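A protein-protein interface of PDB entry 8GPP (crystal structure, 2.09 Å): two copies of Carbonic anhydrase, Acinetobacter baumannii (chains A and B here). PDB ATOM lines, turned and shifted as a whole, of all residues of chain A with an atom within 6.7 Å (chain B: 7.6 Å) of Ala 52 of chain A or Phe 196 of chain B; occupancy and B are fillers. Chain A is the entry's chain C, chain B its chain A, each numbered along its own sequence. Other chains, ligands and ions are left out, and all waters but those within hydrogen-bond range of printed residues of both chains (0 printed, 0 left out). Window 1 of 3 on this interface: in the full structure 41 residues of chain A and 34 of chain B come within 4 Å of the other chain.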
ATOM      1  N   ILE A  13      28.967  19.549  19.847  1.00  0.00           N
ATOM      2  CA  ILE A  13      27.936  20.566  19.988  1.00  0.00           C
ATOM      3  C   ILE A  13      27.420  20.523  21.419  1.00  0.00           C
ATOM      4  O   ILE A  13      27.226  19.443  21.989  1.00  0.00           O
ATOM      5  CB  ILE A  13      26.797  20.392  18.967  1.00  0.00           C
ATOM      6  CG1 ILE A  13      25.868  21.597  19.043  1.00  0.00           C
ATOM      7  CG2 ILE A  13      26.076  19.055  19.152  1.00  0.00           C
ATOM      8  CD1 ILE A  13      24.569  21.393  18.354  1.00  0.00           C
ATOM      9  N   ASP A  14      27.216  21.711  21.998  1.00  0.00           N
ATOM     10  CA  ASP A  14      26.910  21.849  23.419  1.00  0.00           C
ATOM     11  C   ASP A  14      27.933  21.080  24.252  1.00  0.00           C
ATOM     12  O   ASP A  14      27.611  20.461  25.267  1.00  0.00           O
ATOM     13  CB  ASP A  14      25.476  21.397  23.722  1.00  0.00           C
ATOM     14  CG  ASP A  14      24.423  22.376  23.178  1.00  0.00           C
ATOM     15  OD1 ASP A  14      24.718  23.594  23.166  1.00  0.00           O
ATOM     16  OD2 ASP A  14      23.318  21.940  22.751  1.00  0.00           O
ATOM     17  N   GLY A  15      29.189  21.110  23.802  1.00  0.00           N
ATOM     18  CA  GLY A  15      30.252  20.412  24.500  1.00  0.00           C
ATOM     19  C   GLY A  15      30.193  18.898  24.454  1.00  0.00           C
ATOM     20  O   GLY A  15      30.937  18.251  25.199  1.00  0.00           O
ATOM     21  N   VAL A  16      29.345  18.314  23.612  1.00  0.00           N
ATOM     22  CA  VAL A  16      29.237  16.864  23.482  1.00  0.00           C
ATOM     23  C   VAL A  16      30.144  16.390  22.351  1.00  0.00           C
ATOM     24  O   VAL A  16      30.081  16.921  21.231  1.00  0.00           O
ATOM     25  CB  VAL A  16      27.780  16.446  23.240  1.00  0.00           C
ATOM     26  CG1 VAL A  16      27.686  14.968  22.891  1.00  0.00           C
ATOM     27  CG2 VAL A  16      26.951  16.761  24.463  1.00  0.00           C
ATOM     28  N   LEU A  32      31.093  13.381  12.030  1.00  0.00           N
ATOM     29  CA  LEU A  32      30.501  12.919  13.275  1.00  0.00           C
ATOM     30  C   LEU A  32      30.205  14.145  14.122  1.00  0.00           C
ATOM     31  O   LEU A  32      31.117  14.923  14.414  1.00  0.00           O
ATOM     32  CB  LEU A  32      31.454  11.984  14.014  1.00  0.00           C
ATOM     33  CG  LEU A  32      31.296  10.487  13.790  1.00  0.00           C
ATOM     34  CD1 LEU A  32      31.000  10.156  12.350  1.00  0.00           C
ATOM     35  CD2 LEU A  32      32.528   9.742  14.293  1.00  0.00           C
ATOM     36  N   ILE A  33      28.947  14.326  14.507  1.00  0.00           N
ATOM     37  CA  ILE A  33      28.543  15.477  15.310  1.00  0.00           C
ATOM     38  C   ILE A  33      27.900  14.995  16.603  1.00  0.00           C
ATOM     39  O   ILE A  33      26.935  14.221  16.577  1.00  0.00           O
ATOM     40  CB  ILE A  33      27.574  16.397  14.550  1.00  0.00           C
ATOM     41  CG1 ILE A  33      28.338  17.319  13.601  1.00  0.00           C
ATOM     42  CG2 ILE A  33      26.759  17.230  15.541  1.00  0.00           C
ATOM     43  CD1 ILE A  33      27.547  17.707  12.373  1.00  0.00           C
ATOM     44  N   GLY A  34      28.401  15.485  17.721  1.00  0.00           N
ATOM     45  CA  GLY A  34      27.678  15.332  18.982  1.00  0.00           C
ATOM     46  C   GLY A  34      27.802  13.937  19.551  1.00  0.00           C
ATOM     47  O   GLY A  34      28.895  13.375  19.613  1.00  0.00           O
ATOM     48  N   ASP A  35      26.671  13.369  19.979  1.00  0.00           N
ATOM     49  CA  ASP A  35      26.683  12.140  20.783  1.00  0.00           C
ATOM     50  C   ASP A  35      26.604  10.913  19.875  1.00  0.00           C
ATOM     51  O   ASP A  35      25.626  10.157  19.852  1.00  0.00           O
ATOM     52  CB  ASP A  35      25.551  12.157  21.804  1.00  0.00           C
ATOM     53  CG  ASP A  35      25.766  11.149  22.913  1.00  0.00           C
ATOM     54  OD1 ASP A  35      26.746  10.392  22.822  1.00  0.00           O
ATOM     55  OD2 ASP A  35      24.963  11.108  23.868  1.00  0.00           O
ATOM     56  N   VAL A  36      27.659  10.746  19.087  1.00  0.00           N
ATOM     57  CA  VAL A  36      27.843   9.565  18.249  1.00  0.00           C
ATOM     58  C   VAL A  36      28.829   8.666  18.964  1.00  0.00           C
ATOM     59  O   VAL A  36      29.851   9.148  19.470  1.00  0.00           O
ATOM     60  CB  VAL A  36      28.374   9.929  16.853  1.00  0.00           C
ATOM     61  CG1 VAL A  36      28.603   8.648  16.025  1.00  0.00           C
ATOM     62  CG2 VAL A  36      27.450  10.847  16.158  1.00  0.00           C
ATOM     63  N   ILE A  37      28.527   7.373  19.030  1.00  0.00           N
ATOM     64  CA  ILE A  37      29.415   6.396  19.660  1.00  0.00           C
ATOM     65  C   ILE A  37      29.671   5.317  18.624  1.00  0.00           C
ATOM     66  O   ILE A  37      28.737   4.622  18.202  1.00  0.00           O
ATOM     67  CB  ILE A  37      28.835   5.803  20.953  1.00  0.00           C
ATOM     68  CG1 ILE A  37      28.844   6.861  22.054  1.00  0.00           C
ATOM     69  CG2 ILE A  37      29.644   4.547  21.429  1.00  0.00           C
ATOM     70  CD1 ILE A  37      27.603   6.859  22.921  1.00  0.00           C
ATOM     71  N   LEU A  50      26.893  11.305  10.549  1.00  0.00           N
ATOM     72  CA  LEU A  50      26.312  10.769  11.781  1.00  0.00           C
ATOM     73  C   LEU A  50      26.089  11.963  12.695  1.00  0.00           C
ATOM     74  O   LEU A  50      26.992  12.389  13.415  1.00  0.00           O
ATOM     75  CB  LEU A  50      27.215   9.738  12.441  1.00  0.00           C
ATOM     76  CG  LEU A  50      27.906   8.685  11.580  1.00  0.00           C
ATOM     77  CD1 LEU A  50      28.448   7.525  12.448  1.00  0.00           C
ATOM     78  CD2 LEU A  50      26.983   8.169  10.525  1.00  0.00           C
ATOM     79  N   ARG A  51      24.881  12.502  12.663  1.00  0.00           N
ATOM     80  CA  ARG A  51      24.578  13.788  13.292  1.00  0.00           C
ATOM     81  C   ARG A  51      23.751  13.528  14.530  1.00  0.00           C
ATOM     82  O   ARG A  51      22.534  13.367  14.441  1.00  0.00           O
ATOM     83  CB  ARG A  51      23.833  14.711  12.337  1.00  0.00           C
ATOM     84  CG  ARG A  51      23.542  16.096  12.916  1.00  0.00           C
ATOM     85  CD  ARG A  51      23.638  17.144  11.790  1.00  0.00           C
ATOM     86  NE  ARG A  51      22.566  16.992  10.809  1.00  0.00           N
ATOM     87  CZ  ARG A  51      21.373  17.569  10.905  1.00  0.00           C
ATOM     88  NH1 ARG A  51      21.044  18.319  11.953  1.00  0.00           N
ATOM     89  NH2 ARG A  51      20.492  17.404   9.923  1.00  0.00           N
ATOM     90  N   ALA A  52      24.417  13.486  15.676  1.00  0.00           N
ATOM     91  CA  ALA A  52      23.742  13.325  16.963  1.00  0.00           C
ATOM     92  C   ALA A  52      23.649  14.673  17.678  1.00  0.00           C
ATOM     93  O   ALA A  52      24.253  14.894  18.729  1.00  0.00           O
ATOM     94  CB  ALA A  52      24.476  12.286  17.816  1.00  0.00           C
ATOM     95  N   ASP A  53      22.902  15.601  17.077  1.00  0.00           N
ATOM     96  CA  ASP A  53      22.769  16.923  17.680  1.00  0.00           C
ATOM     97  C   ASP A  53      21.449  17.112  18.410  1.00  0.00           C
ATOM     98  O   ASP A  53      21.289  18.111  19.116  1.00  0.00           O
ATOM     99  CB  ASP A  53      22.947  18.037  16.630  1.00  0.00           C
ATOM    100  CG  ASP A  53      22.167  17.786  15.352  1.00  0.00           C
ATOM    101  OD1 ASP A  53      21.305  16.880  15.341  1.00  0.00           O
ATOM    102  OD2 ASP A  53      22.420  18.516  14.357  1.00  0.00           O
ATOM    103  N   PHE A  54      20.516  16.184  18.262  1.00  0.00           N
ATOM    104  CA  PHE A  54      19.287  16.174  19.032  1.00  0.00           C
ATOM    105  C   PHE A  54      19.175  14.955  19.911  1.00  0.00           C
ATOM    106  O   PHE A  54      18.584  15.036  20.986  1.00  0.00           O
ATOM    107  CB  PHE A  54      18.056  16.205  18.115  1.00  0.00           C
ATOM    108  CG  PHE A  54      17.934  17.455  17.301  1.00  0.00           C
ATOM    109  CD1 PHE A  54      17.797  18.687  17.918  1.00  0.00           C
ATOM    110  CD2 PHE A  54      17.954  17.397  15.925  1.00  0.00           C
ATOM    111  CE1 PHE A  54      17.684  19.843  17.172  1.00  0.00           C
ATOM    112  CE2 PHE A  54      17.841  18.549  15.165  1.00  0.00           C
ATOM    113  CZ  PHE A  54      17.703  19.772  15.790  1.00  0.00           C
ATOM    114  N   GLY A  55      19.720  13.828  19.469  1.00  0.00           N
ATOM    115  CA  GLY A  55      19.703  12.600  20.227  1.00  0.00           C
ATOM    116  C   GLY A  55      21.020  11.865  20.100  1.00  0.00           C
ATOM    117  O   GLY A  55      22.024  12.461  19.691  1.00  0.00           O
ATOM    118  N   ARG A  56      21.023  10.576  20.437  1.00  0.00           N
ATOM    119  CA  ARG A  56      22.219   9.750  20.450  1.00  0.00           C
ATOM    120  C   ARG A  56      22.260   8.846  19.223  1.00  0.00           C
ATOM    121  O   ARG A  56      21.224   8.365  18.750  1.00  0.00           O
ATOM    122  CB  ARG A  56      22.273   8.892  21.717  1.00  0.00           C
ATOM    123  CG  ARG A  56      23.419   7.854  21.743  1.00  0.00           C
ATOM    124  CD  ARG A  56      23.581   7.238  23.136  1.00  0.00           C
ATOM    125  NE  ARG A  56      24.173   8.185  24.078  1.00  0.00           N
ATOM    126  CZ  ARG A  56      24.934   7.852  25.112  1.00  0.00           C
ATOM    127  NH1 ARG A  56      25.173   6.582  25.420  1.00  0.00           N
ATOM    128  NH2 ARG A  56      25.470   8.815  25.861  1.00  0.00           N
ATOM    129  N   ILE A  57      23.472   8.611  18.718  1.00  0.00           N
ATOM    130  CA  ILE A  57      23.708   7.615  17.678  1.00  0.00           C
ATOM    131  C   ILE A  57      24.713   6.591  18.204  1.00  0.00           C
ATOM    132  O   ILE A  57      25.800   6.955  18.674  1.00  0.00           O
ATOM    133  CB  ILE A  57      24.192   8.259  16.368  1.00  0.00           C
ATOM    134  CG1 ILE A  57      23.054   9.071  15.738  1.00  0.00           C
ATOM    135  CG2 ILE A  57      24.632   7.179  15.386  1.00  0.00           C
ATOM    136  CD1 ILE A  57      23.497  10.182  14.764  1.00  0.00           C
ATOM    137  N   VAL A  71      22.708   9.592   9.291  1.00  0.00           N
ATOM    138  CA  VAL A  71      22.076   9.101  10.503  1.00  0.00           C
ATOM    139  C   VAL A  71      21.698  10.310  11.357  1.00  0.00           C
ATOM    140  O   VAL A  71      22.521  11.208  11.585  1.00  0.00           O
ATOM    141  CB  VAL A  71      22.994   8.137  11.270  1.00  0.00           C
ATOM    142  CG1 VAL A  71      22.285   7.604  12.505  1.00  0.00           C
ATOM    143  CG2 VAL A  71      23.430   6.998  10.364  1.00  0.00           C
ATOM    144  N   HIS A  72      20.450  10.349  11.798  1.00  0.00           N
ATOM    145  CA  HIS A  72      19.960  11.475  12.578  1.00  0.00           C
ATOM    146  C   HIS A  72      18.750  10.994  13.368  1.00  0.00           C
ATOM    147  O   HIS A  72      18.328   9.842  13.245  1.00  0.00           O
ATOM    148  CB  HIS A  72      19.634  12.656  11.661  1.00  0.00           C
ATOM    149  CG  HIS A  72      19.432  13.954  12.382  1.00  0.00           C
ATOM    150  ND1 HIS A  72      18.237  14.633  12.360  1.00  0.00           N
ATOM    151  CD2 HIS A  72      20.277  14.708  13.127  1.00  0.00           C
ATOM    152  CE1 HIS A  72      18.346  15.748  13.063  1.00  0.00           C
ATOM    153  NE2 HIS A  72      19.576  15.816  13.541  1.00  0.00           N
ATOM    154  N   GLY A  73      18.195  11.879  14.186  1.00  0.00           N
ATOM    155  CA  GLY A  73      17.052  11.529  15.013  1.00  0.00           C
ATOM    156  C   GLY A  73      16.561  12.768  15.721  1.00  0.00           C
ATOM    157  O   GLY A  73      17.271  13.781  15.793  1.00  0.00           O
ATOM    158  N   GLN A  76      16.125  13.799  21.963  1.00  0.00           N
ATOM    159  CA  GLN A  76      16.147  12.722  22.940  1.00  0.00           C
ATOM    160  C   GLN A  76      16.102  11.341  22.297  1.00  0.00           C
ATOM    161  O   GLN A  76      16.143  10.346  23.018  1.00  0.00           O
ATOM    162  CB  GLN A  76      15.000  12.865  23.944  1.00  0.00           C
ATOM    163  CG  GLN A  76      15.264  13.960  24.976  1.00  0.00           C
ATOM    164  CD  GLN A  76      16.757  14.198  25.220  1.00  0.00           C
ATOM    165  OE1 GLN A  76      17.398  15.039  24.563  1.00  0.00           O
ATOM    166  NE2 GLN A  76      17.313  13.469  26.200  1.00  0.00           N
ATOM    167  N   GLU B 168      16.756  26.871  16.140  1.00  0.00           N
ATOM    168  CA  GLU B 168      17.557  26.799  17.357  1.00  0.00           C
ATOM    169  C   GLU B 168      18.906  26.141  17.082  1.00  0.00           C
ATOM    170  O   GLU B 168      19.950  26.613  17.551  1.00  0.00           O
ATOM    171  CB  GLU B 168      16.771  26.011  18.403  1.00  0.00           C
ATOM    172  CG  GLU B 168      17.289  26.000  19.810  1.00  0.00           C
ATOM    173  CD  GLU B 168      16.415  25.122  20.697  1.00  0.00           C
ATOM    174  OE1 GLU B 168      15.197  25.001  20.384  1.00  0.00           O
ATOM    175  OE2 GLU B 168      16.938  24.557  21.689  1.00  0.00           O
ATOM    176  N   LEU B 169      18.902  25.066  16.284  1.00  0.00           N
ATOM    177  CA  LEU B 169      20.142  24.365  15.954  1.00  0.00           C
ATOM    178  C   LEU B 169      21.143  25.303  15.295  1.00  0.00           C
ATOM    179  O   LEU B 169      22.335  25.294  15.631  1.00  0.00           O
ATOM    180  CB  LEU B 169      19.852  23.179  15.029  1.00  0.00           C
ATOM    181  CG  LEU B 169      21.078  22.404  14.511  1.00  0.00           C
ATOM    182  CD1 LEU B 169      21.863  21.748  15.663  1.00  0.00           C
ATOM    183  CD2 LEU B 169      20.696  21.354  13.439  1.00  0.00           C
ATOM    184  N   ARG B 172      22.614  27.183  18.063  1.00  0.00           N
ATOM    185  CA  ARG B 172      23.504  26.318  18.834  1.00  0.00           C
ATOM    186  C   ARG B 172      24.829  26.102  18.110  1.00  0.00           C
ATOM    187  O   ARG B 172      25.901  26.149  18.733  1.00  0.00           O
ATOM    188  CB  ARG B 172      22.824  24.973  19.119  1.00  0.00           C
ATOM    189  CG  ARG B 172      21.688  25.024  20.136  1.00  0.00           C
ATOM    190  CD  ARG B 172      20.902  23.712  20.192  1.00  0.00           C
ATOM    191  NE  ARG B 172      21.721  22.573  20.600  1.00  0.00           N
ATOM    192  CZ  ARG B 172      21.545  21.330  20.168  1.00  0.00           C
ATOM    193  NH1 ARG B 172      20.589  21.028  19.306  1.00  0.00           N
ATOM    194  NH2 ARG B 172      22.357  20.368  20.603  1.00  0.00           N
ATOM    195  N   LEU B 191      29.951  14.571  28.585  1.00  0.00           N
ATOM    196  CA  LEU B 191      28.684  15.171  28.194  1.00  0.00           C
ATOM    197  C   LEU B 191      27.974  14.276  27.180  1.00  0.00           C
ATOM    198  O   LEU B 191      28.610  13.552  26.406  1.00  0.00           O
ATOM    199  CB  LEU B 191      28.936  16.555  27.606  1.00  0.00           C
ATOM    200  CG  LEU B 191      28.914  17.710  28.610  1.00  0.00           C
ATOM    201  CD1 LEU B 191      29.672  18.890  28.037  1.00  0.00           C
ATOM    202  CD2 LEU B 191      27.499  18.114  28.942  1.00  0.00           C
ATOM    203  N   THR B 192      26.638  14.312  27.198  1.00  0.00           N
ATOM    204  CA  THR B 192      25.825  13.446  26.351  1.00  0.00           C
ATOM    205  C   THR B 192      24.672  14.257  25.788  1.00  0.00           C
ATOM    206  O   THR B 192      24.515  15.442  26.098  1.00  0.00           O
ATOM    207  CB  THR B 192      25.257  12.245  27.118  1.00  0.00           C
ATOM    208  OG1 THR B 192      24.249  12.699  28.026  1.00  0.00           O
ATOM    209  CG2 THR B 192      26.354  11.529  27.915  1.00  0.00           C
ATOM    210  N   TYR B 193      23.843  13.601  24.967  1.00  0.00           N
ATOM    211  CA  TYR B 193      22.656  14.256  24.427  1.00  0.00           C
ATOM    212  C   TYR B 193      21.699  14.717  25.519  1.00  0.00           C
ATOM    213  O   TYR B 193      20.894  15.625  25.274  1.00  0.00           O
ATOM    214  CB  TYR B 193      21.912  13.322  23.480  1.00  0.00           C
ATOM    215  CG  TYR B 193      21.217  12.189  24.194  1.00  0.00           C
ATOM    216  CD1 TYR B 193      21.910  11.046  24.566  1.00  0.00           C
ATOM    217  CD2 TYR B 193      19.866  12.255  24.492  1.00  0.00           C
ATOM    218  CE1 TYR B 193      21.277  10.003  25.223  1.00  0.00           C
ATOM    219  CE2 TYR B 193      19.227  11.216  25.155  1.00  0.00           C
ATOM    220  CZ  TYR B 193      19.937  10.095  25.511  1.00  0.00           C
ATOM    221  OH  TYR B 193      19.291   9.071  26.153  1.00  0.00           O
ATOM    222  N   LYS B 194      21.750  14.092  26.708  1.00  0.00           N
ATOM    223  CA  LYS B 194      20.942  14.543  27.831  1.00  0.00           C
ATOM    224  C   LYS B 194      21.319  15.949  28.264  1.00  0.00           C
ATOM    225  O   LYS B 194      20.548  16.600  28.977  1.00  0.00           O
ATOM    226  CB  LYS B 194      21.103  13.561  29.003  1.00  0.00           C
ATOM    227  CG  LYS B 194      20.730  12.109  28.657  1.00  0.00           C
ATOM    228  CD  LYS B 194      21.042  11.153  29.798  1.00  0.00           C
ATOM    229  CE  LYS B 194      22.402  10.491  29.630  1.00  0.00           C
ATOM    230  NZ  LYS B 194      22.507   9.214  30.437  1.00  0.00           N
ATOM    231  N   ASP B 195      22.487  16.427  27.853  1.00  0.00           N
ATOM    232  CA  ASP B 195      22.939  17.790  28.093  1.00  0.00           C
ATOM    233  C   ASP B 195      22.572  18.758  26.971  1.00  0.00           C
ATOM    234  O   ASP B 195      22.968  19.927  27.030  1.00  0.00           O
ATOM    235  CB  ASP B 195      24.450  17.798  28.306  1.00  0.00           C
ATOM    236  CG  ASP B 195      24.862  16.990  29.514  1.00  0.00           C
ATOM    237  OD1 ASP B 195      24.750  17.527  30.636  1.00  0.00           O
ATOM    238  OD2 ASP B 195      25.297  15.828  29.343  1.00  0.00           O
ATOM    239  N   PHE B 196      21.809  18.332  25.986  1.00  0.00           N
ATOM    240  CA  PHE B 196      21.425  19.228  24.921  1.00  0.00           C
ATOM    241  C   PHE B 196      20.302  20.133  25.395  1.00  0.00           C
ATOM    242  O   PHE B 196      19.612  19.843  26.349  1.00  0.00           O
ATOM    243  CB  PHE B 196      20.893  18.454  23.730  1.00  0.00           C
ATOM    244  CG  PHE B 196      21.936  17.794  22.913  1.00  0.00           C
ATOM    245  CD1 PHE B 196      23.210  18.238  22.918  1.00  0.00           C
ATOM    246  CD2 PHE B 196      21.621  16.728  22.138  1.00  0.00           C
ATOM    247  CE1 PHE B 196      24.158  17.629  22.158  1.00  0.00           C
ATOM    248  CE2 PHE B 196      22.565  16.101  21.390  1.00  0.00           C
ATOM    249  CZ  PHE B 196      23.833  16.557  21.396  1.00  0.00           C
ATOM    250  N   SER B 197      20.093  21.218  24.679  1.00  0.00           N
ATOM    251  CA  SER B 197      19.021  22.132  24.985  1.00  0.00           C
ATOM    252  C   SER B 197      17.777  21.615  24.281  1.00  0.00           C
ATOM    253  O   SER B 197      17.211  20.595  24.646  1.00  0.00           O
ATOM    254  CB  SER B 197      19.345  23.549  24.485  1.00  0.00           C
ATOM    255  OG  SER B 197      20.727  23.737  24.241  1.00  0.00           O
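NE of Arg 172 of chain B is in salt-bridge range of OD2 of Asp 14 of chain A (2.8 Å).
NH2 of Arg 172 of chain B lies within hydrogen-bond range of O of Asp 53 of chain A.
The backbone NH of Tyr 193 of chain B is in hydrogen-bond range of the side-chain carboxylate of Asp 35 of chain A.
OD2 of Asp 14 of chain A lies within hydrogen-bond range of OG of Ser 197 of chain B, at 3.5 Å.
The backbone NH of Lys 194 of chain B sits close to the side-chain hydroxyl of Thr 192 of chain B (3.2 Å).
N of Thr 192 of chain B sits at hydrogen-bond distance from OD2 of Asp 195 of chain B (2.9 Å).
NE of Arg 56 of chain A lies within salt-bridge range of OD2 of Asp 35 of chain A (3.0 Å).
N of Ile 57 of chain A sits at hydrogen-bond distance from O of Asp 35 of chain A, at 2.9 Å.
The backbone NH (N) of Arg 51 of chain A is in hydrogen-bond range of the backbone carbonyl oxygen (O) of Val 71 of chain A, 2.9 Å away.
O of Phe 54 of chain A is in hydrogen-bond range of N of Gln 76 of chain A (2.9 Å).
Among the printed residues, merely in contact across the chains: Gln 76 of chain A with Tyr 193 of chain B (3.1 Å), Ala 52 of chain A with Phe 196 of chain B (3.2 Å), Gly 15 of chain A with Leu 191 of chain B (3.2 Å), Val 16 of chain A with Thr 192 of chain B (3.2 Å), Asp 53 of chain A with Phe 196 of chain B (3.3 Å), Ile 13 of chain A with Arg 172 of chain B (3.3 Å), Arg 51 of chain A with Leu 169 of chain B (3.4 Å), Asp 53 of chain A with Leu 169 of chain B (3.4 Å), Asp 35 of chain A with Thr 192 of chain B (3.5 Å), Arg 56 of chain A with Thr 192 of chain B (3.5 Å), Ile 13 of chain A with Phe 196 of chain B (3.6 Å), Arg 56 of chain A with Tyr 193 of chain B (3.6 Å), Phe 54 of chain A with Phe 196 of chain B (3.7 Å), Asp 14 of chain A with Phe 196 of chain B (3.7 Å), Val 16 of chain A with Leu 191 of chain B (3.7 Å), Val 16 of chain A with Phe 196 of chain B (3.7 Å), Gly 55 of chain A with Tyr 193 of chain B (3.8 Å), Asp 14 of chain A with Leu 191 of chain B (3.8 Å), Phe 54 of chain A with Arg 172 of chain B (3.8 Å) and Ile 13 of chain A with Leu 169 of chain B (3.8 Å).
Of the printed residues of chain B, Gly 15 of chain A touches Leu 191 (3.2 Å).
Of chain B, only Phe 196 comes within 4 Å of Ala 52 of chain A.
Of the printed residues of chain A, Leu 191 of chain B touches Asp 14, Gly 15 and Val 16.
Phe 196 of chain B touches six residues of chain A.
The nearest residue of chain B that does not touch Ala 52 of chain A is Tyr 193 of chain B (5.5 Å).
The nearest residue of chain A that does not touch Phe 196 of chain B is Gly 55 of chain A (4.1 Å).
The nearest printed residue of chain B that does not touch Arg 51 of chain A is Phe 196 of chain B (7.4 Å).
Hydrophobic or aromatic side chains of chain B that line the printed part of chain A: Leu 169, Leu 191, Tyr 193 and Phe 196.
Along chain B the printed residues that touch a printed residue of chain A span positions 169 to 197.
Of the 22 printed residues of chain A, 12 touch a printed residue of chain B.
Among the printed residues, 24 pairs touch across the chains.
No position is printed for both chains.
Of the 24 pairs that touch across the chains among the printed residues, none has its exchanged pair printed and touching as well.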
